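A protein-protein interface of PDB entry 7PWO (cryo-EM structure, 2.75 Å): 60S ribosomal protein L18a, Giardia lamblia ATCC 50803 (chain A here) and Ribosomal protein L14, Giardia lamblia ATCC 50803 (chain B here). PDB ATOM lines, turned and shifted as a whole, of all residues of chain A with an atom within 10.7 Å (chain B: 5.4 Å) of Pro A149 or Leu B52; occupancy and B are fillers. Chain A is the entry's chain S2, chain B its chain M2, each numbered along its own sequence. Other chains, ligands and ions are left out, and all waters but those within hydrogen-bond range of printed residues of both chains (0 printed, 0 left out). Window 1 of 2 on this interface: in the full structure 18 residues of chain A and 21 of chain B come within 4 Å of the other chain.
O of Phe A146 is in hydrogen-bond range of N of Val B7 (2.6 Å). The backbone carbonyl oxygen (O) of Leu B52 sits at hydrogen-bond distance from a ring nitrogen (NE2) of His A148. O of Arg B53 lies close to NE2 of His A154. O of Arg B53 is in hydrogen-bond range of NH2 of Arg A157, at 3.2 Å. O of Ala B55 sits at hydrogen-bond distance from NE2 of His A148 (3.3 Å). O of Ala B55 lies close to NE2 of His A154, 3.4 Å away.
Of chain B, only Thr B33 (3.7 Å) and Leu B52 (3.9 Å) come within 4 Å of Pro A149. Leu B52 touches three residues of chain A. Thr B33 touches just these residues of chain A: Phe A139 (3.4 Å) and Pro A149 (3.7 Å). No residue of chain A comes within 4 Å of Ala B34. No residue of chain A comes within 4 Å of Ser B51. Of chain A, only His A148 (3.3 Å) and His A154 (3.0 Å) come within 4 Å of Ala B55. Of the printed residues of chain B, Cys A150 touches Arg B53. Of the printed residues of chain A, Ser B32 touches Phe A139 and Phe A146. Of the printed residues of chain B, Arg A145 touches Val B7. Printed residues of chain B within 4 Å of Phe A139: Ser B32 and Thr B33. Of the printed residues of chain B, His A154 touches Leu B52 (3.7 Å), Arg B53 (3.4 Å) and Ala B55 (3.0 Å). The nearest residue of chain A that does not touch Leu B52 is Phe A146 (4.2 Å). The nearest printed residue of chain B that does not touch Cys A150 is Leu B52 (5.2 Å).
OG of Ser B32 sits close to N of Ala B34 (3.4 Å). N of Leu B52 sits at hydrogen-bond distance from O of Ala B34, 3.1 Å away. The side-chain hydroxyl (OG) of Ser B51 lies close to the backbone NH (N) of Arg B53. A ring nitrogen (ND1) of His A148 is in hydrogen-bond range of the backbone NH of Cys A150, 3.2 Å away.
Phe A139 touches Ser B32. Phe A139 touches Thr B33. Val A144 touches Val B7 (O to O, 3.6 Å). Arg A145 touches Val B7. O of Ser B32 touches CZ of Phe A146 (3.96 Å). O of Thr B33 touches CG of Pro A149 (3.7 Å). Leu B52 touches Pro A149. CG of Arg B53 touches SG of Cys A150, 3.9 Å away. Arg B53 touches Val A153. Leu B52 touches His A154.
Of the 17 printed residues of chain A, 10 touch a printed residue of chain B. Hydrophobic or aromatic side chains of chain A within 4 Å of the printed part of chain B: Phe A139, Phe A146, His A148, Pro A149, Val A153 and His A154. Printed residues of chain B that touch a printed residue of chain A: Val B7, Ser B32, Thr B33, Leu B52, Arg B53 and Ala B55. Hydrophobic or aromatic side chains of chain B that line the printed part of chain A: Val B7 and Leu B52. Among the printed residues, 16 pairs touch across the chains. Among the printed residues, no Asp or Glu carboxylate lies within 4 Å of a Lys or Arg side-chain nitrogen of the other chain.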
ATOM      1  N   PHE A 139      11.658   4.248 -37.072  1.00  0.00           N
ATOM      2  CA  PHE A 139      12.749   3.484 -37.649  1.00  0.00           C
ATOM      3  C   PHE A 139      13.281   4.090 -38.937  1.00  0.00           C
ATOM      4  O   PHE A 139      14.253   3.573 -39.494  1.00  0.00           O
ATOM      5  CB  PHE A 139      12.281   2.049 -37.890  1.00  0.00           C
ATOM      6  CG  PHE A 139      11.992   1.298 -36.636  1.00  0.00           C
ATOM      7  CD1 PHE A 139      13.017   0.709 -35.924  1.00  0.00           C
ATOM      8  CD2 PHE A 139      10.703   1.215 -36.140  1.00  0.00           C
ATOM      9  CE1 PHE A 139      12.761   0.034 -34.764  1.00  0.00           C
ATOM     10  CE2 PHE A 139      10.448   0.539 -34.977  1.00  0.00           C
ATOM     11  CZ  PHE A 139      11.478  -0.051 -34.290  1.00  0.00           C
ATOM     12  N   VAL A 144      19.371   4.472 -35.024  1.00  0.00           N
ATOM     13  CA  VAL A 144      18.375   3.939 -34.102  1.00  0.00           C
ATOM     14  C   VAL A 144      18.970   2.754 -33.348  1.00  0.00           C
ATOM     15  O   VAL A 144      19.541   1.838 -33.951  1.00  0.00           O
ATOM     16  CB  VAL A 144      17.078   3.568 -34.844  1.00  0.00           C
ATOM     17  CG1 VAL A 144      17.290   2.432 -35.830  1.00  0.00           C
ATOM     18  CG2 VAL A 144      15.981   3.221 -33.853  1.00  0.00           C
ATOM     19  N   ARG A 145      18.878   2.794 -32.018  1.00  0.00           N
ATOM     20  CA  ARG A 145      19.411   1.757 -31.143  1.00  0.00           C
ATOM     21  C   ARG A 145      18.391   1.389 -30.084  1.00  0.00           C
ATOM     22  O   ARG A 145      17.711   2.257 -29.530  1.00  0.00           O
ATOM     23  CB  ARG A 145      20.683   2.195 -30.420  1.00  0.00           C
ATOM     24  CG  ARG A 145      21.592   3.113 -31.188  1.00  0.00           C
ATOM     25  CD  ARG A 145      22.767   3.535 -30.331  1.00  0.00           C
ATOM     26  NE  ARG A 145      23.741   2.469 -30.135  1.00  0.00           N
ATOM     27  CZ  ARG A 145      24.217   2.100 -28.951  1.00  0.00           C
ATOM     28  NH1 ARG A 145      23.828   2.723 -27.849  1.00  0.00           N
ATOM     29  NH2 ARG A 145      25.100   1.118 -28.872  1.00  0.00           N
ATOM     30  N   PHE A 146      18.312   0.100 -29.783  1.00  0.00           N
ATOM     31  CA  PHE A 146      17.551  -0.361 -28.639  1.00  0.00           C
ATOM     32  C   PHE A 146      18.153  -1.659 -28.128  1.00  0.00           C
ATOM     33  O   PHE A 146      18.731  -2.424 -28.908  1.00  0.00           O
ATOM     34  CB  PHE A 146      16.057  -0.522 -28.969  1.00  0.00           C
ATOM     35  CG  PHE A 146      15.771  -1.215 -30.281  1.00  0.00           C
ATOM     36  CD1 PHE A 146      15.775  -0.498 -31.471  1.00  0.00           C
ATOM     37  CD2 PHE A 146      15.450  -2.559 -30.321  1.00  0.00           C
ATOM     38  CE1 PHE A 146      15.498  -1.114 -32.674  1.00  0.00           C
ATOM     39  CE2 PHE A 146      15.173  -3.183 -31.529  1.00  0.00           C
ATOM     40  CZ  PHE A 146      15.195  -2.463 -32.701  1.00  0.00           C
ATOM     41  N   PRO A 147      18.087  -1.904 -26.826  1.00  0.00           N
ATOM     42  CA  PRO A 147      18.497  -3.206 -26.303  1.00  0.00           C
ATOM     43  C   PRO A 147      17.483  -4.266 -26.681  1.00  0.00           C
ATOM     44  O   PRO A 147      16.312  -3.966 -26.924  1.00  0.00           O
ATOM     45  CB  PRO A 147      18.538  -2.981 -24.790  1.00  0.00           C
ATOM     46  CG  PRO A 147      17.584  -1.879 -24.549  1.00  0.00           C
ATOM     47  CD  PRO A 147      17.583  -1.010 -25.773  1.00  0.00           C
ATOM     48  N   HIS A 148      17.938  -5.519 -26.709  1.00  0.00           N
ATOM     49  CA  HIS A 148      17.127  -6.603 -27.237  1.00  0.00           C
ATOM     50  C   HIS A 148      15.780  -6.660 -26.519  1.00  0.00           C
ATOM     51  O   HIS A 148      15.741  -6.681 -25.283  1.00  0.00           O
ATOM     52  CB  HIS A 148      17.855  -7.938 -27.096  1.00  0.00           C
ATOM     53  CG  HIS A 148      17.377  -8.995 -28.042  1.00  0.00           C
ATOM     54  ND1 HIS A 148      16.062  -9.397 -28.103  1.00  0.00           N
ATOM     55  CD2 HIS A 148      18.037  -9.735 -28.961  1.00  0.00           C
ATOM     56  CE1 HIS A 148      15.932 -10.340 -29.016  1.00  0.00           C
ATOM     57  NE2 HIS A 148      17.115 -10.563 -29.553  1.00  0.00           N
ATOM     58  N   PRO A 149      14.662  -6.662 -27.252  1.00  0.00           N
ATOM     59  CA  PRO A 149      13.348  -6.566 -26.604  1.00  0.00           C
ATOM     60  C   PRO A 149      12.830  -7.857 -25.993  1.00  0.00           C
ATOM     61  O   PRO A 149      11.784  -7.815 -25.336  1.00  0.00           O
ATOM     62  CB  PRO A 149      12.434  -6.099 -27.746  1.00  0.00           C
ATOM     63  CG  PRO A 149      13.135  -6.486 -28.992  1.00  0.00           C
ATOM     64  CD  PRO A 149      14.592  -6.447 -28.706  1.00  0.00           C
ATOM     65  N   CYS A 150      13.507  -8.992 -26.165  1.00  0.00           N
ATOM     66  CA  CYS A 150      13.008 -10.221 -25.555  1.00  0.00           C
ATOM     67  C   CYS A 150      14.077 -11.303 -25.442  1.00  0.00           C
ATOM     68  O   CYS A 150      13.949 -12.361 -26.066  1.00  0.00           O
ATOM     69  CB  CYS A 150      11.798 -10.738 -26.345  1.00  0.00           C
ATOM     70  SG  CYS A 150      12.090 -11.113 -28.091  1.00  0.00           S
ATOM     71  N   PRO A 151      15.120 -11.108 -24.632  1.00  0.00           N
ATOM     72  CA  PRO A 151      16.216 -12.085 -24.589  1.00  0.00           C
ATOM     73  C   PRO A 151      15.958 -13.304 -23.711  1.00  0.00           C
ATOM     74  O   PRO A 151      16.826 -14.173 -23.631  1.00  0.00           O
ATOM     75  CB  PRO A 151      17.391 -11.254 -24.054  1.00  0.00           C
ATOM     76  CG  PRO A 151      16.757 -10.096 -23.324  1.00  0.00           C
ATOM     77  CD  PRO A 151      15.308 -10.018 -23.663  1.00  0.00           C
ATOM     78  N   TYR A 152      14.805 -13.397 -23.048  1.00  0.00           N
ATOM     79  CA  TYR A 152      14.436 -14.610 -22.326  1.00  0.00           C
ATOM     80  C   TYR A 152      14.137 -15.768 -23.271  1.00  0.00           C
ATOM     81  O   TYR A 152      14.192 -16.935 -22.855  1.00  0.00           O
ATOM     82  CB  TYR A 152      13.199 -14.359 -21.461  1.00  0.00           C
ATOM     83  CG  TYR A 152      11.973 -13.979 -22.258  1.00  0.00           C
ATOM     84  CD1 TYR A 152      11.860 -12.746 -22.861  1.00  0.00           C
ATOM     85  CD2 TYR A 152      10.939 -14.883 -22.436  1.00  0.00           C
ATOM     86  CE1 TYR A 152      10.746 -12.412 -23.592  1.00  0.00           C
ATOM     87  CE2 TYR A 152       9.818 -14.553 -23.167  1.00  0.00           C
ATOM     88  CZ  TYR A 152       9.734 -13.320 -23.750  1.00  0.00           C
ATOM     89  OH  TYR A 152       8.623 -12.976 -24.486  1.00  0.00           O
ATOM     90  N   VAL A 153      13.795 -15.451 -24.521  1.00  0.00           N
ATOM     91  CA  VAL A 153      13.289 -16.438 -25.464  1.00  0.00           C
ATOM     92  C   VAL A 153      14.373 -17.447 -25.809  1.00  0.00           C
ATOM     93  O   VAL A 153      14.112 -18.654 -25.892  1.00  0.00           O
ATOM     94  CB  VAL A 153      12.738 -15.718 -26.714  1.00  0.00           C
ATOM     95  CG1 VAL A 153      12.310 -16.692 -27.772  1.00  0.00           C
ATOM     96  CG2 VAL A 153      11.577 -14.808 -26.333  1.00  0.00           C
ATOM     97  N   HIS A 154      15.612 -16.973 -25.978  1.00  0.00           N
ATOM     98  CA  HIS A 154      16.741 -17.861 -26.239  1.00  0.00           C
ATOM     99  C   HIS A 154      16.941 -18.853 -25.105  1.00  0.00           C
ATOM    100  O   HIS A 154      17.158 -20.050 -25.337  1.00  0.00           O
ATOM    101  CB  HIS A 154      18.009 -17.030 -26.428  1.00  0.00           C
ATOM    102  CG  HIS A 154      17.886 -15.968 -27.474  1.00  0.00           C
ATOM    103  ND1 HIS A 154      18.745 -14.895 -27.545  1.00  0.00           N
ATOM    104  CD2 HIS A 154      17.005 -15.811 -28.487  1.00  0.00           C
ATOM    105  CE1 HIS A 154      18.394 -14.120 -28.554  1.00  0.00           C
ATOM    106  NE2 HIS A 154      17.343 -14.656 -29.144  1.00  0.00           N
ATOM    107  N   VAL A 155      16.868 -18.365 -23.866  1.00  0.00           N
ATOM    108  CA  VAL A 155      17.133 -19.196 -22.699  1.00  0.00           C
ATOM    109  C   VAL A 155      16.067 -20.277 -22.568  1.00  0.00           C
ATOM    110  O   VAL A 155      16.377 -21.460 -22.367  1.00  0.00           O
ATOM    111  CB  VAL A 155      17.208 -18.314 -21.438  1.00  0.00           C
ATOM    112  CG1 VAL A 155      17.561 -19.127 -20.208  1.00  0.00           C
ATOM    113  CG2 VAL A 155      18.163 -17.159 -21.640  1.00  0.00           C
ATOM    114  N   ARG A 157      14.189 -21.461 -24.968  1.00  0.00           N
ATOM    115  CA  ARG A 157      14.314 -22.384 -26.086  1.00  0.00           C
ATOM    116  C   ARG A 157      15.387 -23.428 -25.811  1.00  0.00           C
ATOM    117  O   ARG A 157      15.176 -24.621 -26.046  1.00  0.00           O
ATOM    118  CB  ARG A 157      14.614 -21.603 -27.363  1.00  0.00           C
ATOM    119  CG  ARG A 157      14.304 -22.354 -28.633  1.00  0.00           C
ATOM    120  CD  ARG A 157      15.211 -21.909 -29.763  1.00  0.00           C
ATOM    121  NE  ARG A 157      15.367 -20.457 -29.815  1.00  0.00           N
ATOM    122  CZ  ARG A 157      16.530 -19.826 -29.704  1.00  0.00           C
ATOM    123  NH1 ARG A 157      17.647 -20.510 -29.507  1.00  0.00           N
ATOM    124  NH2 ARG A 157      16.578 -18.506 -29.774  1.00  0.00           N
ATOM    125  N   VAL A 171      20.448 -14.180 -18.035  1.00  0.00           N
ATOM    126  CA  VAL A 171      19.845 -13.661 -19.260  1.00  0.00           C
ATOM    127  C   VAL A 171      20.714 -12.498 -19.727  1.00  0.00           C
ATOM    128  O   VAL A 171      20.502 -11.360 -19.292  1.00  0.00           O
ATOM    129  CB  VAL A 171      18.383 -13.240 -19.031  1.00  0.00           C
ATOM    130  CG1 VAL A 171      17.788 -12.620 -20.284  1.00  0.00           C
ATOM    131  CG2 VAL A 171      17.546 -14.405 -18.533  1.00  0.00           C
ATOM    132  N   PRO A 172      21.712 -12.736 -20.583  1.00  0.00           N
ATOM    133  CA  PRO A 172      22.682 -11.683 -20.925  1.00  0.00           C
ATOM    134  C   PRO A 172      22.045 -10.522 -21.674  1.00  0.00           C
ATOM    135  O   PRO A 172      21.382 -10.708 -22.697  1.00  0.00           O
ATOM    136  CB  PRO A 172      23.701 -12.411 -21.810  1.00  0.00           C
ATOM    137  CG  PRO A 172      23.453 -13.850 -21.617  1.00  0.00           C
ATOM    138  CD  PRO A 172      22.027 -14.011 -21.239  1.00  0.00           C
ATOM    139  N   GLN A 173      22.275  -9.313 -21.165  1.00  0.00           N
ATOM    140  CA  GLN A 173      21.764  -8.090 -21.773  1.00  0.00           C
ATOM    141  C   GLN A 173      22.819  -6.992 -21.822  1.00  0.00           C
ATOM    142  O   GLN A 173      24.019  -7.263 -21.890  1.00  0.00           O
ATOM    143  CB  GLN A 173      20.543  -7.586 -21.013  1.00  0.00           C
ATOM    144  CG  GLN A 173      19.634  -8.681 -20.560  1.00  0.00           C
ATOM    145  CD  GLN A 173      18.407  -8.171 -19.869  1.00  0.00           C
ATOM    146  OE1 GLN A 173      17.862  -7.131 -20.230  1.00  0.00           O
ATOM    147  NE2 GLN A 173      17.952  -8.910 -18.870  1.00  0.00           N
ATOM    148  N   VAL B   7      20.678  -3.331 -30.342  1.00  0.00           N
ATOM    149  CA  VAL B   7      20.277  -3.630 -31.711  1.00  0.00           C
ATOM    150  C   VAL B   7      20.569  -2.394 -32.553  1.00  0.00           C
ATOM    151  O   VAL B   7      20.060  -1.305 -32.265  1.00  0.00           O
ATOM    152  CB  VAL B   7      18.787  -4.005 -31.783  1.00  0.00           C
ATOM    153  CG1 VAL B   7      18.359  -4.219 -33.220  1.00  0.00           C
ATOM    154  CG2 VAL B   7      18.498  -5.222 -30.960  1.00  0.00           C
ATOM    155  N   SER B  32      11.537  -3.147 -37.497  1.00  0.00           N
ATOM    156  CA  SER B  32      10.706  -2.688 -36.394  1.00  0.00           C
ATOM    157  C   SER B  32      11.242  -3.329 -35.121  1.00  0.00           C
ATOM    158  O   SER B  32      12.360  -3.851 -35.095  1.00  0.00           O
ATOM    159  CB  SER B  32       9.231  -3.014 -36.640  1.00  0.00           C
ATOM    160  OG  SER B  32       8.983  -4.409 -36.604  1.00  0.00           O
ATOM    161  N   THR B  33      10.454  -3.298 -34.070  1.00  0.00           N
ATOM    162  CA  THR B  33      10.913  -3.956 -32.855  1.00  0.00           C
ATOM    163  C   THR B  33      10.800  -5.483 -32.925  1.00  0.00           C
ATOM    164  O   THR B  33      10.939  -6.109 -31.885  1.00  0.00           O
ATOM    165  CB  THR B  33      10.140  -3.434 -31.643  1.00  0.00           C
ATOM    166  OG1 THR B  33       8.729  -3.509 -31.893  1.00  0.00           O
ATOM    167  CG2 THR B  33      10.525  -1.987 -31.343  1.00  0.00           C
ATOM    168  N   ALA B  34      10.565  -6.115 -34.078  1.00  0.00           N
ATOM    169  CA  ALA B  34      10.506  -7.566 -34.157  1.00  0.00           C
ATOM    170  C   ALA B  34      11.371  -8.187 -35.247  1.00  0.00           C
ATOM    171  O   ALA B  34      11.467  -9.416 -35.286  1.00  0.00           O
ATOM    172  CB  ALA B  34       9.059  -8.036 -34.373  1.00  0.00           C
ATOM    173  N   ALA B  35      11.985  -7.402 -36.131  1.00  0.00           N
ATOM    174  CA  ALA B  35      12.609  -7.976 -37.312  1.00  0.00           C
ATOM    175  C   ALA B  35      13.790  -7.135 -37.774  1.00  0.00           C
ATOM    176  O   ALA B  35      13.784  -5.901 -37.687  1.00  0.00           O
ATOM    177  CB  ALA B  35      11.604  -8.115 -38.458  1.00  0.00           C
ATOM    178  N   VAL B  36      14.794  -7.825 -38.305  1.00  0.00           N
ATOM    179  CA  VAL B  36      15.963  -7.172 -38.870  1.00  0.00           C
ATOM    180  C   VAL B  36      16.275  -7.779 -40.227  1.00  0.00           C
ATOM    181  O   VAL B  36      15.857  -8.891 -40.554  1.00  0.00           O
ATOM    182  CB  VAL B  36      17.202  -7.262 -37.946  1.00  0.00           C
ATOM    183  CG1 VAL B  36      16.953  -6.562 -36.635  1.00  0.00           C
ATOM    184  CG2 VAL B  36      17.550  -8.703 -37.678  1.00  0.00           C
ATOM    185  N   VAL B  50      15.136 -11.744 -40.605  1.00  0.00           N
ATOM    186  CA  VAL B  50      14.903 -12.670 -39.508  1.00  0.00           C
ATOM    187  C   VAL B  50      14.164 -11.966 -38.379  1.00  0.00           C
ATOM    188  O   VAL B  50      14.155 -10.739 -38.255  1.00  0.00           O
ATOM    189  CB  VAL B  50      16.207 -13.311 -38.985  1.00  0.00           C
ATOM    190  CG1 VAL B  50      16.923 -14.052 -40.100  1.00  0.00           C
ATOM    191  CG2 VAL B  50      17.110 -12.255 -38.358  1.00  0.00           C
ATOM    192  N   SER B  51      13.499 -12.784 -37.574  1.00  0.00           N
ATOM    193  CA  SER B  51      12.917 -12.356 -36.311  1.00  0.00           C
ATOM    194  C   SER B  51      14.006 -12.204 -35.252  1.00  0.00           C
ATOM    195  O   SER B  51      14.921 -13.024 -35.165  1.00  0.00           O
ATOM    196  CB  SER B  51      11.883 -13.389 -35.863  1.00  0.00           C
ATOM    197  OG  SER B  51      11.292 -13.067 -34.627  1.00  0.00           O
ATOM    198  N   LEU B  52      13.894 -11.157 -34.428  1.00  0.00           N
ATOM    199  CA  LEU B  52      14.841 -10.980 -33.329  1.00  0.00           C
ATOM    200  C   LEU B  52      14.818 -12.136 -32.344  1.00  0.00           C
ATOM    201  O   LEU B  52      15.788 -12.327 -31.605  1.00  0.00           O
ATOM    202  CB  LEU B  52      14.570  -9.670 -32.591  1.00  0.00           C
ATOM    203  CG  LEU B  52      14.831  -8.403 -33.396  1.00  0.00           C
ATOM    204  CD1 LEU B  52      14.400  -7.171 -32.640  1.00  0.00           C
ATOM    205  CD2 LEU B  52      16.313  -8.337 -33.656  1.00  0.00           C
ATOM    206  N   ARG B  53      13.753 -12.928 -32.340  1.00  0.00           N
ATOM    207  CA  ARG B  53      13.652 -14.092 -31.483  1.00  0.00           C
ATOM    208  C   ARG B  53      14.673 -15.175 -31.841  1.00  0.00           C
ATOM    209  O   ARG B  53      14.855 -16.109 -31.055  1.00  0.00           O
ATOM    210  CB  ARG B  53      12.221 -14.620 -31.563  1.00  0.00           C
ATOM    211  CG  ARG B  53      11.228 -13.773 -30.779  1.00  0.00           C
ATOM    212  CD  ARG B  53       9.777 -14.228 -30.902  1.00  0.00           C
ATOM    213  NE  ARG B  53       9.593 -15.663 -30.729  1.00  0.00           N
ATOM    214  CZ  ARG B  53       8.993 -16.203 -29.677  1.00  0.00           C
ATOM    215  NH1 ARG B  53       8.546 -15.427 -28.709  1.00  0.00           N
ATOM    216  NH2 ARG B  53       8.864 -17.515 -29.575  1.00  0.00           N
ATOM    217  N   TRP B  54      15.345 -15.075 -32.993  1.00  0.00           N
ATOM    218  CA  TRP B  54      16.359 -16.050 -33.402  1.00  0.00           C
ATOM    219  C   TRP B  54      17.795 -15.560 -33.266  1.00  0.00           C
ATOM    220  O   TRP B  54      18.716 -16.369 -33.398  1.00  0.00           O
ATOM    221  CB  TRP B  54      16.164 -16.477 -34.860  1.00  0.00           C
ATOM    222  CG  TRP B  54      14.933 -17.217 -35.185  1.00  0.00           C
ATOM    223  CD1 TRP B  54      13.989 -17.660 -34.326  1.00  0.00           C
ATOM    224  CD2 TRP B  54      14.498 -17.594 -36.490  1.00  0.00           C
ATOM    225  NE1 TRP B  54      12.997 -18.311 -35.006  1.00  0.00           N
ATOM    226  CE2 TRP B  54      13.286 -18.279 -36.341  1.00  0.00           C
ATOM    227  CE3 TRP B  54      15.020 -17.418 -37.772  1.00  0.00           C
ATOM    228  CZ2 TRP B  54      12.584 -18.790 -37.424  1.00  0.00           C
ATOM    229  CZ3 TRP B  54      14.326 -17.919 -38.839  1.00  0.00           C
ATOM    230  CH2 TRP B  54      13.117 -18.600 -38.662  1.00  0.00           C
ATOM    231  N   ALA B  55      18.021 -14.276 -33.028  1.00  0.00           N
ATOM    232  CA  ALA B  55      19.349 -13.686 -33.109  1.00  0.00           C
ATOM    233  C   ALA B  55      19.867 -13.394 -31.712  1.00  0.00           C
ATOM    234  O   ALA B  55      19.297 -12.560 -31.005  1.00  0.00           O
ATOM    235  CB  ALA B  55      19.312 -12.412 -33.945  1.00  0.00           C
